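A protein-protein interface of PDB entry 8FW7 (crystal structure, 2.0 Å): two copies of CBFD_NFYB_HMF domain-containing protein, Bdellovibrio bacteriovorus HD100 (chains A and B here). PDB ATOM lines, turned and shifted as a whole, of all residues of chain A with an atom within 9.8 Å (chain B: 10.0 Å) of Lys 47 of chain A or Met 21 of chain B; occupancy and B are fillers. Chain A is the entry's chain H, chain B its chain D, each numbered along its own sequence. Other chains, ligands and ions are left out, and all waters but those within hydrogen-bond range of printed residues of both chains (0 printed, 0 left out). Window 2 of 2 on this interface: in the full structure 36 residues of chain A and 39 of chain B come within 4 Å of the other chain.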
ATOM      1  N   CYS A  39     -16.768 -14.742  27.716  1.00  0.00           N
ATOM      2  CA  CYS A  39     -15.707 -14.390  26.772  1.00  0.00           C
ATOM      3  C   CYS A  39     -16.063 -13.138  25.975  1.00  0.00           C
ATOM      4  O   CYS A  39     -15.202 -12.279  25.742  1.00  0.00           O
ATOM      5  CB  CYS A  39     -15.402 -15.565  25.834  1.00  0.00           C
ATOM      6  SG  CYS A  39     -14.796 -17.085  26.633  1.00  0.00           S
ATOM      7  N   LEU A  40     -17.312 -13.022  25.529  1.00  0.00           N
ATOM      8  CA  LEU A  40     -17.730 -11.832  24.789  1.00  0.00           C
ATOM      9  C   LEU A  40     -17.558 -10.566  25.628  1.00  0.00           C
ATOM     10  O   LEU A  40     -17.128  -9.523  25.115  1.00  0.00           O
ATOM     11  CB  LEU A  40     -19.186 -11.971  24.327  1.00  0.00           C
ATOM     12  CG  LEU A  40     -19.476 -12.568  22.944  1.00  0.00           C
ATOM     13  CD1 LEU A  40     -18.955 -11.645  21.839  1.00  0.00           C
ATOM     14  CD2 LEU A  40     -18.899 -13.953  22.791  1.00  0.00           C
ATOM     15  N   LYS A  41     -17.878 -10.636  26.923  1.00  0.00           N
ATOM     16  CA  LYS A  41     -17.661  -9.478  27.787  1.00  0.00           C
ATOM     17  C   LYS A  41     -16.174  -9.239  28.024  1.00  0.00           C
ATOM     18  O   LYS A  41     -15.731  -8.086  28.089  1.00  0.00           O
ATOM     19  CB  LYS A  41     -18.404  -9.653  29.108  1.00  0.00           C
ATOM     20  CG  LYS A  41     -19.896  -9.338  29.013  1.00  0.00           C
ATOM     21  CD  LYS A  41     -20.697  -9.986  30.141  1.00  0.00           C
ATOM     22  CE  LYS A  41     -21.869  -9.112  30.576  1.00  0.00           C
ATOM     23  NZ  LYS A  41     -21.498  -8.123  31.624  1.00  0.00           N
ATOM     24  N   GLY A  42     -15.386 -10.313  28.139  1.00  0.00           N
ATOM     25  CA  GLY A  42     -13.947 -10.152  28.275  1.00  0.00           C
ATOM     26  C   GLY A  42     -13.323  -9.446  27.085  1.00  0.00           C
ATOM     27  O   GLY A  42     -12.401  -8.637  27.239  1.00  0.00           O
ATOM     28  N   VAL A  43     -13.817  -9.741  25.879  1.00  0.00           N
ATOM     29  CA  VAL A  43     -13.288  -9.099  24.681  1.00  0.00           C
ATOM     30  C   VAL A  43     -13.649  -7.616  24.670  1.00  0.00           C
ATOM     31  O   VAL A  43     -12.831  -6.763  24.300  1.00  0.00           O
ATOM     32  CB  VAL A  43     -13.802  -9.823  23.423  1.00  0.00           C
ATOM     33  CG1 VAL A  43     -13.747  -8.899  22.204  1.00  0.00           C
ATOM     34  CG2 VAL A  43     -13.018 -11.101  23.181  1.00  0.00           C
ATOM     35  N   GLU A  44     -14.878  -7.285  25.075  1.00  0.00           N
ATOM     36  CA  GLU A  44     -15.270  -5.884  25.169  1.00  0.00           C
ATOM     37  C   GLU A  44     -14.490  -5.167  26.269  1.00  0.00           C
ATOM     38  O   GLU A  44     -14.160  -3.982  26.124  1.00  0.00           O
ATOM     39  CB  GLU A  44     -16.781  -5.781  25.392  1.00  0.00           C
ATOM     40  CG  GLU A  44     -17.474  -4.655  24.601  1.00  0.00           C
ATOM     41  CD  GLU A  44     -17.443  -4.849  23.077  1.00  0.00           C
ATOM     42  OE1 GLU A  44     -17.170  -5.978  22.610  1.00  0.00           O
ATOM     43  OE2 GLU A  44     -17.689  -3.861  22.341  1.00  0.00           O
ATOM     44  N   SER A  45     -14.146  -5.874  27.351  1.00  0.00           N
ATOM     45  CA  SER A  45     -13.361  -5.262  28.421  1.00  0.00           C
ATOM     46  C   SER A  45     -11.916  -5.031  27.997  1.00  0.00           C
ATOM     47  O   SER A  45     -11.318  -4.015  28.372  1.00  0.00           O
ATOM     48  CB  SER A  45     -13.418  -6.128  29.680  1.00  0.00           C
ATOM     49  OG  SER A  45     -12.378  -5.783  30.583  1.00  0.00           O
ATOM     50  N   ALA A  46     -11.338  -5.943  27.215  1.00  0.00           N
ATOM     51  CA  ALA A  46      -9.984  -5.713  26.720  1.00  0.00           C
ATOM     52  C   ALA A  46      -9.957  -4.596  25.680  1.00  0.00           C
ATOM     53  O   ALA A  46      -9.060  -3.744  25.702  1.00  0.00           O
ATOM     54  CB  ALA A  46      -9.406  -7.006  26.149  1.00  0.00           C
ATOM     55  N   LYS A  47     -10.939  -4.578  24.768  1.00  0.00           N
ATOM     56  CA  LYS A  47     -10.989  -3.542  23.740  1.00  0.00           C
ATOM     57  C   LYS A  47     -11.139  -2.155  24.356  1.00  0.00           C
ATOM     58  O   LYS A  47     -10.484  -1.201  23.924  1.00  0.00           O
ATOM     59  CB  LYS A  47     -12.132  -3.822  22.766  1.00  0.00           C
ATOM     60  CG  LYS A  47     -11.812  -3.493  21.308  1.00  0.00           C
ATOM     61  CD  LYS A  47     -10.411  -3.974  20.924  1.00  0.00           C
ATOM     62  CE  LYS A  47     -10.232  -4.120  19.420  1.00  0.00           C
ATOM     63  NZ  LYS A  47      -9.159  -5.109  19.118  1.00  0.00           N
ATOM     64  N   ALA A  48     -11.990  -2.026  25.374  1.00  0.00           N
ATOM     65  CA  ALA A  48     -12.136  -0.760  26.079  1.00  0.00           C
ATOM     66  C   ALA A  48     -10.839  -0.298  26.743  1.00  0.00           C
ATOM     67  O   ALA A  48     -10.734   0.881  27.101  1.00  0.00           O
ATOM     68  CB  ALA A  48     -13.247  -0.873  27.124  1.00  0.00           C
ATOM     69  N   ASP A  49      -9.857  -1.184  26.915  1.00  0.00           N
ATOM     70  CA  ASP A  49      -8.549  -0.829  27.453  1.00  0.00           C
ATOM     71  C   ASP A  49      -7.466  -0.811  26.381  1.00  0.00           C
ATOM     72  O   ASP A  49      -6.283  -0.663  26.711  1.00  0.00           O
ATOM     73  CB  ASP A  49      -8.148  -1.796  28.572  1.00  0.00           C
ATOM     74  CG  ASP A  49      -7.129  -1.196  29.535  1.00  0.00           C
ATOM     75  OD1 ASP A  49      -7.219   0.021  29.811  1.00  0.00           O
ATOM     76  OD2 ASP A  49      -6.226  -1.939  29.994  1.00  0.00           O
ATOM     77  N   GLY A  50      -7.835  -0.983  25.113  1.00  0.00           N
ATOM     78  CA  GLY A  50      -6.859  -0.978  24.036  1.00  0.00           C
ATOM     79  C   GLY A  50      -5.855  -2.107  24.086  1.00  0.00           C
ATOM     80  O   GLY A  50      -4.707  -1.929  23.653  1.00  0.00           O
ATOM     81  N   ARG A  51      -6.248  -3.269  24.605  1.00  0.00           N
ATOM     82  CA  ARG A  51      -5.391  -4.443  24.625  1.00  0.00           C
ATOM     83  C   ARG A  51      -5.868  -5.459  23.595  1.00  0.00           C
ATOM     84  O   ARG A  51      -7.002  -5.409  23.112  1.00  0.00           O
ATOM     85  CB  ARG A  51      -5.356  -5.082  26.019  1.00  0.00           C
ATOM     86  CG  ARG A  51      -4.676  -4.234  27.081  1.00  0.00           C
ATOM     87  CD  ARG A  51      -4.639  -4.968  28.413  1.00  0.00           C
ATOM     88  NE  ARG A  51      -5.875  -4.772  29.164  1.00  0.00           N
ATOM     89  CZ  ARG A  51      -6.861  -5.658  29.247  1.00  0.00           C
ATOM     90  NH1 ARG A  51      -6.785  -6.842  28.656  1.00  0.00           N
ATOM     91  NH2 ARG A  51      -7.953  -5.349  29.945  1.00  0.00           N
ATOM     92  N   LYS A  52      -4.971  -6.387  23.261  1.00  0.00           N
ATOM     93  CA  LYS A  52      -5.211  -7.422  22.263  1.00  0.00           C
ATOM     94  C   LYS A  52      -5.314  -8.810  22.881  1.00  0.00           C
ATOM     95  O   LYS A  52      -5.255  -9.810  22.156  1.00  0.00           O
ATOM     96  CB  LYS A  52      -4.096  -7.417  21.212  1.00  0.00           C
ATOM     97  CG  LYS A  52      -3.830  -6.069  20.572  1.00  0.00           C
ATOM     98  CD  LYS A  52      -4.953  -5.666  19.631  1.00  0.00           C
ATOM     99  CE  LYS A  52      -4.720  -4.262  19.101  1.00  0.00           C
ATOM    100  NZ  LYS A  52      -4.432  -4.274  17.638  1.00  0.00           N
ATOM    101  N   THR A  53      -5.437  -8.895  24.203  1.00  0.00           N
ATOM    102  CA  THR A  53      -5.420 -10.169  24.911  1.00  0.00           C
ATOM    103  C   THR A  53      -6.457 -10.109  26.016  1.00  0.00           C
ATOM    104  O   THR A  53      -6.445  -9.178  26.832  1.00  0.00           O
ATOM    105  CB  THR A  53      -4.036 -10.463  25.505  1.00  0.00           C
ATOM    106  OG1 THR A  53      -3.078 -10.597  24.448  1.00  0.00           O
ATOM    107  CG2 THR A  53      -4.065 -11.748  26.325  1.00  0.00           C
ATOM    108  N   VAL A  54      -7.359 -11.090  26.038  1.00  0.00           N
ATOM    109  CA  VAL A  54      -8.253 -11.244  27.176  1.00  0.00           C
ATOM    110  C   VAL A  54      -7.467 -11.807  28.349  1.00  0.00           C
ATOM    111  O   VAL A  54      -6.829 -12.864  28.244  1.00  0.00           O
ATOM    112  CB  VAL A  54      -9.435 -12.153  26.815  1.00  0.00           C
ATOM    113  CG1 VAL A  54     -10.395 -12.247  27.981  1.00  0.00           C
ATOM    114  CG2 VAL A  54     -10.120 -11.639  25.570  1.00  0.00           C
ATOM    115  N   MET A  55      -7.526 -11.119  29.479  1.00  0.00           N
ATOM    116  CA  MET A  55      -6.830 -11.533  30.687  1.00  0.00           C
ATOM    117  C   MET A  55      -7.840 -11.901  31.763  1.00  0.00           C
ATOM    118  O   MET A  55      -9.029 -11.595  31.661  1.00  0.00           O
ATOM    119  CB  MET A  55      -5.902 -10.418  31.190  1.00  0.00           C
ATOM    120  CG  MET A  55      -5.239  -9.648  30.073  1.00  0.00           C
ATOM    121  SD  MET A  55      -3.511  -9.343  30.457  1.00  0.00           S
ATOM    122  CE  MET A  55      -2.806 -10.944  30.090  1.00  0.00           C
ATOM    123  N   ASP A  58     -10.206  -9.431  32.839  1.00  0.00           N
ATOM    124  CA  ASP A  58     -11.316  -9.125  31.942  1.00  0.00           C
ATOM    125  C   ASP A  58     -12.522 -10.028  32.146  1.00  0.00           C
ATOM    126  O   ASP A  58     -13.566  -9.783  31.530  1.00  0.00           O
ATOM    127  CB  ASP A  58     -10.858  -9.223  30.487  1.00  0.00           C
ATOM    128  CG  ASP A  58      -9.854  -8.152  30.132  1.00  0.00           C
ATOM    129  OD1 ASP A  58     -10.055  -7.004  30.585  1.00  0.00           O
ATOM    130  OD2 ASP A  58      -8.859  -8.452  29.429  1.00  0.00           O
ATOM    131  N   SER B   9      -9.168 -24.923  23.655  1.00  0.00           N
ATOM    132  CA  SER B   9      -8.996 -24.636  22.230  1.00  0.00           C
ATOM    133  C   SER B   9     -10.195 -23.887  21.659  1.00  0.00           C
ATOM    134  O   SER B   9     -10.031 -22.970  20.845  1.00  0.00           O
ATOM    135  CB  SER B   9      -8.759 -25.935  21.460  1.00  0.00           C
ATOM    136  OG  SER B   9      -9.749 -26.886  21.793  1.00  0.00           O
ATOM    137  N   LYS B  10     -11.413 -24.250  22.084  1.00  0.00           N
ATOM    138  CA  LYS B  10     -12.604 -23.577  21.567  1.00  0.00           C
ATOM    139  C   LYS B  10     -12.817 -22.215  22.214  1.00  0.00           C
ATOM    140  O   LYS B  10     -13.395 -21.317  21.586  1.00  0.00           O
ATOM    141  CB  LYS B  10     -13.858 -24.435  21.778  1.00  0.00           C
ATOM    142  CG  LYS B  10     -13.714 -25.921  21.453  1.00  0.00           C
ATOM    143  CD  LYS B  10     -13.867 -26.222  19.973  1.00  0.00           C
ATOM    144  CE  LYS B  10     -14.420 -27.634  19.780  1.00  0.00           C
ATOM    145  NZ  LYS B  10     -13.476 -28.671  20.286  1.00  0.00           N
ATOM    146  N   VAL B  11     -12.397 -22.051  23.469  1.00  0.00           N
ATOM    147  CA  VAL B  11     -12.454 -20.728  24.089  1.00  0.00           C
ATOM    148  C   VAL B  11     -11.536 -19.766  23.336  1.00  0.00           C
ATOM    149  O   VAL B  11     -11.956 -18.681  22.911  1.00  0.00           O
ATOM    150  CB  VAL B  11     -12.092 -20.822  25.582  1.00  0.00           C
ATOM    151  CG1 VAL B  11     -11.741 -19.434  26.146  1.00  0.00           C
ATOM    152  CG2 VAL B  11     -13.256 -21.460  26.364  1.00  0.00           C
ATOM    153  N   LYS B  12     -10.282 -20.178  23.128  1.00  0.00           N
ATOM    154  CA  LYS B  12      -9.336 -19.359  22.377  1.00  0.00           C
ATOM    155  C   LYS B  12      -9.832 -19.092  20.965  1.00  0.00           C
ATOM    156  O   LYS B  12      -9.702 -17.972  20.453  1.00  0.00           O
ATOM    157  CB  LYS B  12      -7.968 -20.041  22.325  1.00  0.00           C
ATOM    158  CG  LYS B  12      -7.305 -20.188  23.676  1.00  0.00           C
ATOM    159  CD  LYS B  12      -5.797 -20.119  23.565  1.00  0.00           C
ATOM    160  CE  LYS B  12      -5.120 -21.034  24.572  1.00  0.00           C
ATOM    161  NZ  LYS B  12      -4.161 -21.979  23.919  1.00  0.00           N
ATOM    162  N   LYS B  13     -10.389 -20.117  20.310  1.00  0.00           N
ATOM    163  CA  LYS B  13     -10.846 -19.947  18.936  1.00  0.00           C
ATOM    164  C   LYS B  13     -12.004 -18.963  18.866  1.00  0.00           C
ATOM    165  O   LYS B  13     -12.080 -18.148  17.939  1.00  0.00           O
ATOM    166  CB  LYS B  13     -11.233 -21.305  18.346  1.00  0.00           C
ATOM    167  CG  LYS B  13     -11.938 -21.255  17.005  1.00  0.00           C
ATOM    168  CD  LYS B  13     -12.631 -22.576  16.727  1.00  0.00           C
ATOM    169  CE  LYS B  13     -11.695 -23.543  16.028  1.00  0.00           C
ATOM    170  NZ  LYS B  13     -12.385 -24.819  15.704  1.00  0.00           N
ATOM    171  N   LEU B  14     -12.905 -19.006  19.849  1.00  0.00           N
ATOM    172  CA  LEU B  14     -14.020 -18.067  19.866  1.00  0.00           C
ATOM    173  C   LEU B  14     -13.541 -16.643  20.126  1.00  0.00           C
ATOM    174  O   LEU B  14     -14.057 -15.689  19.535  1.00  0.00           O
ATOM    175  CB  LEU B  14     -15.044 -18.510  20.912  1.00  0.00           C
ATOM    176  CG  LEU B  14     -16.074 -17.511  21.424  1.00  0.00           C
ATOM    177  CD1 LEU B  14     -17.291 -17.502  20.521  1.00  0.00           C
ATOM    178  CD2 LEU B  14     -16.475 -17.864  22.856  1.00  0.00           C
ATOM    179  N   ILE B  15     -12.539 -16.479  20.993  1.00  0.00           N
ATOM    180  CA  ILE B  15     -12.048 -15.141  21.313  1.00  0.00           C
ATOM    181  C   ILE B  15     -11.264 -14.557  20.141  1.00  0.00           C
ATOM    182  O   ILE B  15     -11.370 -13.360  19.836  1.00  0.00           O
ATOM    183  CB  ILE B  15     -11.208 -15.188  22.600  1.00  0.00           C
ATOM    184  CG1 ILE B  15     -12.127 -15.275  23.820  1.00  0.00           C
ATOM    185  CG2 ILE B  15     -10.319 -13.965  22.720  1.00  0.00           C
ATOM    186  CD1 ILE B  15     -11.433 -15.842  25.025  1.00  0.00           C
ATOM    187  N   LYS B  16     -10.467 -15.385  19.461  1.00  0.00           N
ATOM    188  CA  LYS B  16      -9.759 -14.897  18.283  1.00  0.00           C
ATOM    189  C   LYS B  16     -10.719 -14.658  17.122  1.00  0.00           C
ATOM    190  O   LYS B  16     -10.593 -13.665  16.401  1.00  0.00           O
ATOM    191  CB  LYS B  16      -8.647 -15.875  17.891  1.00  0.00           C
ATOM    192  CG  LYS B  16      -7.512 -15.222  17.095  1.00  0.00           C
ATOM    193  CD  LYS B  16      -6.199 -15.995  17.227  1.00  0.00           C
ATOM    194  CE  LYS B  16      -5.140 -15.458  16.274  1.00  0.00           C
ATOM    195  NZ  LYS B  16      -5.081 -16.275  15.023  1.00  0.00           N
ATOM    196  N   GLU B  17     -11.711 -15.533  16.949  1.00  0.00           N
ATOM    197  CA  GLU B  17     -12.611 -15.429  15.803  1.00  0.00           C
ATOM    198  C   GLU B  17     -13.642 -14.319  15.978  1.00  0.00           C
ATOM    199  O   GLU B  17     -14.091 -13.735  14.985  1.00  0.00           O
ATOM    200  CB  GLU B  17     -13.315 -16.771  15.579  1.00  0.00           C
ATOM    201  CG  GLU B  17     -13.830 -17.028  14.173  1.00  0.00           C
ATOM    202  CD  GLU B  17     -13.888 -18.515  13.840  1.00  0.00           C
ATOM    203  OE1 GLU B  17     -12.956 -19.258  14.226  1.00  0.00           O
ATOM    204  OE2 GLU B  17     -14.880 -18.946  13.210  1.00  0.00           O
ATOM    205  N   LYS B  18     -14.027 -14.008  17.217  1.00  0.00           N
ATOM    206  CA  LYS B  18     -15.036 -12.988  17.473  1.00  0.00           C
ATOM    207  C   LYS B  18     -14.461 -11.651  17.924  1.00  0.00           C
ATOM    208  O   LYS B  18     -15.182 -10.648  17.890  1.00  0.00           O
ATOM    209  CB  LYS B  18     -16.037 -13.476  18.529  1.00  0.00           C
ATOM    210  CG  LYS B  18     -16.944 -14.601  18.060  1.00  0.00           C
ATOM    211  CD  LYS B  18     -18.249 -14.050  17.511  1.00  0.00           C
ATOM    212  CE  LYS B  18     -19.333 -14.031  18.582  1.00  0.00           C
ATOM    213  NZ  LYS B  18     -19.620 -15.392  19.124  1.00  0.00           N
ATOM    214  N   GLY B  19     -13.200 -11.602  18.348  1.00  0.00           N
ATOM    215  CA  GLY B  19     -12.627 -10.348  18.798  1.00  0.00           C
ATOM    216  C   GLY B  19     -11.223 -10.083  18.286  1.00  0.00           C
ATOM    217  O   GLY B  19     -10.665  -9.004  18.525  1.00  0.00           O
ATOM    218  N   GLN B  20     -10.646 -11.062  17.588  1.00  0.00           N
ATOM    219  CA  GLN B  20      -9.293 -11.028  17.032  1.00  0.00           C
ATOM    220  C   GLN B  20      -8.207 -11.041  18.096  1.00  0.00           C
ATOM    221  O   GLN B  20      -7.033 -10.791  17.778  1.00  0.00           O
ATOM    222  CB  GLN B  20      -9.067  -9.821  16.114  1.00  0.00           C
ATOM    223  CG  GLN B  20      -9.652  -9.961  14.722  1.00  0.00           C
ATOM    224  CD  GLN B  20     -10.814  -9.018  14.494  1.00  0.00           C
ATOM    225  OE1 GLN B  20     -11.514  -8.644  15.434  1.00  0.00           O
ATOM    226  NE2 GLN B  20     -11.009  -8.607  13.243  1.00  0.00           N
ATOM    227  N   MET B  21      -8.543 -11.341  19.343  1.00  0.00           N
ATOM    228  CA  MET B  21      -7.567 -11.240  20.414  1.00  0.00           C
ATOM    229  C   MET B  21      -7.002 -12.602  20.791  1.00  0.00           C
ATOM    230  O   MET B  21      -7.532 -13.654  20.422  1.00  0.00           O
ATOM    231  CB  MET B  21      -8.184 -10.576  21.647  1.00  0.00           C
ATOM    232  CG  MET B  21      -9.188  -9.494  21.328  1.00  0.00           C
ATOM    233  SD  MET B  21      -9.643  -8.597  22.818  1.00  0.00           S
ATOM    234  CE  MET B  21     -10.446  -7.165  22.114  1.00  0.00           C
ATOM    235  N   ASN B  22      -5.896 -12.560  21.524  1.00  0.00           N
ATOM    236  CA  ASN B  22      -5.374 -13.736  22.190  1.00  0.00           C
ATOM    237  C   ASN B  22      -6.061 -13.932  23.542  1.00  0.00           C
ATOM    238  O   ASN B  22      -6.862 -13.110  23.997  1.00  0.00           O
ATOM    239  CB  ASN B  22      -3.861 -13.633  22.373  1.00  0.00           C
ATOM    240  CG  ASN B  22      -3.122 -13.451  21.055  1.00  0.00           C
ATOM    241  OD1 ASN B  22      -3.593 -13.882  20.004  1.00  0.00           O
ATOM    242  ND2 ASN B  22      -1.951 -12.827  21.113  1.00  0.00           N
ATOM    243  N   THR B  23      -5.732 -15.050  24.181  1.00  0.00           N
ATOM    244  CA  THR B  23      -6.316 -15.447  25.456  1.00  0.00           C
ATOM    245  C   THR B  23      -5.175 -15.778  26.400  1.00  0.00           C
ATOM    246  O   THR B  23      -4.373 -16.674  26.112  1.00  0.00           O
ATOM    247  CB  THR B  23      -7.234 -16.667  25.295  1.00  0.00           C
ATOM    248  OG1 THR B  23      -8.317 -16.351  24.412  1.00  0.00           O
ATOM    249  CG2 THR B  23      -7.788 -17.096  26.648  1.00  0.00           C
ATOM    250  N   SER B  24      -5.090 -15.058  27.513  1.00  0.00           N
ATOM    251  CA  SER B  24      -4.047 -15.360  28.483  1.00  0.00           C
ATOM    252  C   SER B  24      -4.289 -16.719  29.147  1.00  0.00           C
ATOM    253  O   SER B  24      -5.397 -17.267  29.132  1.00  0.00           O
ATOM    254  CB  SER B  24      -3.968 -14.267  29.545  1.00  0.00           C
ATOM    255  OG  SER B  24      -4.957 -14.457  30.547  1.00  0.00           O
ATOM    256  N   THR B  27      -6.795 -16.683  32.137  1.00  0.00           N
ATOM    257  CA  THR B  27      -8.188 -16.510  31.712  1.00  0.00           C
ATOM    258  C   THR B  27      -8.926 -17.842  31.736  1.00  0.00           C
ATOM    259  O   THR B  27     -10.088 -17.915  32.159  1.00  0.00           O
ATOM    260  CB  THR B  27      -8.257 -15.911  30.304  1.00  0.00           C
ATOM    261  OG1 THR B  27      -7.751 -14.566  30.308  1.00  0.00           O
ATOM    262  CG2 THR B  27      -9.699 -15.899  29.795  1.00  0.00           C
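The backbone carbonyl oxygen (O) of Lys 52 of chain A is in hydrogen-bond range of the backbone NH (N) of Asn 22 of chain B. N of Val 54 of chain A lies within hydrogen-bond range of O of Asn 22 of chain B (2.9 Å). O of Val 54 of chain A is in hydrogen-bond range of N of Ser 24 of chain B (2.9 Å). The side-chain hydroxyl (OG1) of Thr 27 of chain B sits at hydrogen-bond distance from the backbone carbonyl oxygen (O) of Val 54 of chain A, 2.8 Å away.
Cys 39 of chain A touches Ile 15 of chain B. CG2 of Val 43 of chain A touches CG2 of Ile 15 of chain B, 3.96 Å away. CG1 of Val 43 of chain A touches CA of Gly 19 of chain B, at 3.9 Å. Met 21 of chain B touches Val 43 of chain A. CB of Ala 46 of chain A touches SD of Met 21 of chain B, 3.7 Å away. Met 21 of chain B touches Arg 51 of chain A. Lys 52 of chain A touches Met 21 of chain B. CG2 of Thr 53 of chain A touches N of Ser 24 of chain B (3.7 Å). CA of Met 55 of chain A touches OG of Ser 24 of chain B, at 3.5 Å. Met 55 of chain A touches Thr 27 of chain B.
No position is printed for both chains.
Printed residues of chain A that touch a printed residue of chain B: Cys 39, Val 43, Ala 46, Lys 47, Arg 51, Lys 52, Thr 53, Val 54 and Met 55. Hydrophobic or aromatic side chains of chain A that line the printed part of chain B: Val 43, Ala 46, Val 54 and Met 55. Among the printed residues, no Asp or Glu carboxylate lies within 4 Å of a Lys or Arg side-chain nitrogen of the other chain.
Of chain B, only Met 21 comes within 4 Å of Lys 47 of chain A. Of the printed residues of chain A, Met 21 of chain B touches Val 43 (3.3 Å), Ala 46 (3.7 Å), Lys 47 (3.4 Å), Arg 51 (3.99 Å) and Lys 52 (3.1 Å). Glu 44 of chain A touches none of the printed residues of chain B. Of chain B, only Met 21 (3.7 Å) comes within 4 Å of Ala 46 of chain A. Ala 48 of chain A touches none of the printed residues of chain B. No residue of chain B comes within 4 Å of Gly 50 of chain A. Of the printed residues of chain B, Lys 52 of chain A touches Met 21 and Asn 22. Of chain A, only Val 43 comes within 4 Å of Gly 19 of chain B. Of the printed residues of chain A, Asn 22 of chain B touches Lys 52 (2.9 Å), Thr 53 (3.4 Å) and Val 54 (2.9 Å). Of the printed residues of chain A, Thr 27 of chain B touches Val 54 and Met 55. Of the printed residues of chain A, Ile 15 of chain B touches Cys 39 (3.9 Å), Val 43 (3.96 Å) and Val 54 (3.7 Å). Asp 58 of chain A touches none of the printed residues of chain B. The nearest printed residue of chain A that does not touch Met 21 of chain B is Thr 53 of chain A (4.1 Å).
The backbone carbonyl oxygen (O) of Ile 15 of chain B is in hydrogen-bond range of the backbone NH (N) of Gln 20 of chain B (3.3 Å). The side-chain hydroxyl (OG1) of Thr 27 of chain B sits at hydrogen-bond distance from the side-chain hydroxyl (OG) of Ser 24 of chain B (2.8 Å). The backbone carbonyl oxygen (O) of Ala 46 of chain A lies within hydrogen-bond range of the backbone NH (N) of Arg 51 of chain A. The guanidinium group (NH1) of Arg 51 of chain A sits at hydrogen-bond distance from the backbone carbonyl oxygen (O) of Thr 53 of chain A, 3.0 Å away. NH1 of Arg 51 of chain A is in salt-bridge range of OD2 of Asp 58 of chain A, at 2.7 Å. The backbone NH of Met 55 of chain A is in hydrogen-bond range of the side-chain carboxylate of Asp 58 of chain A (3.0 Å).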
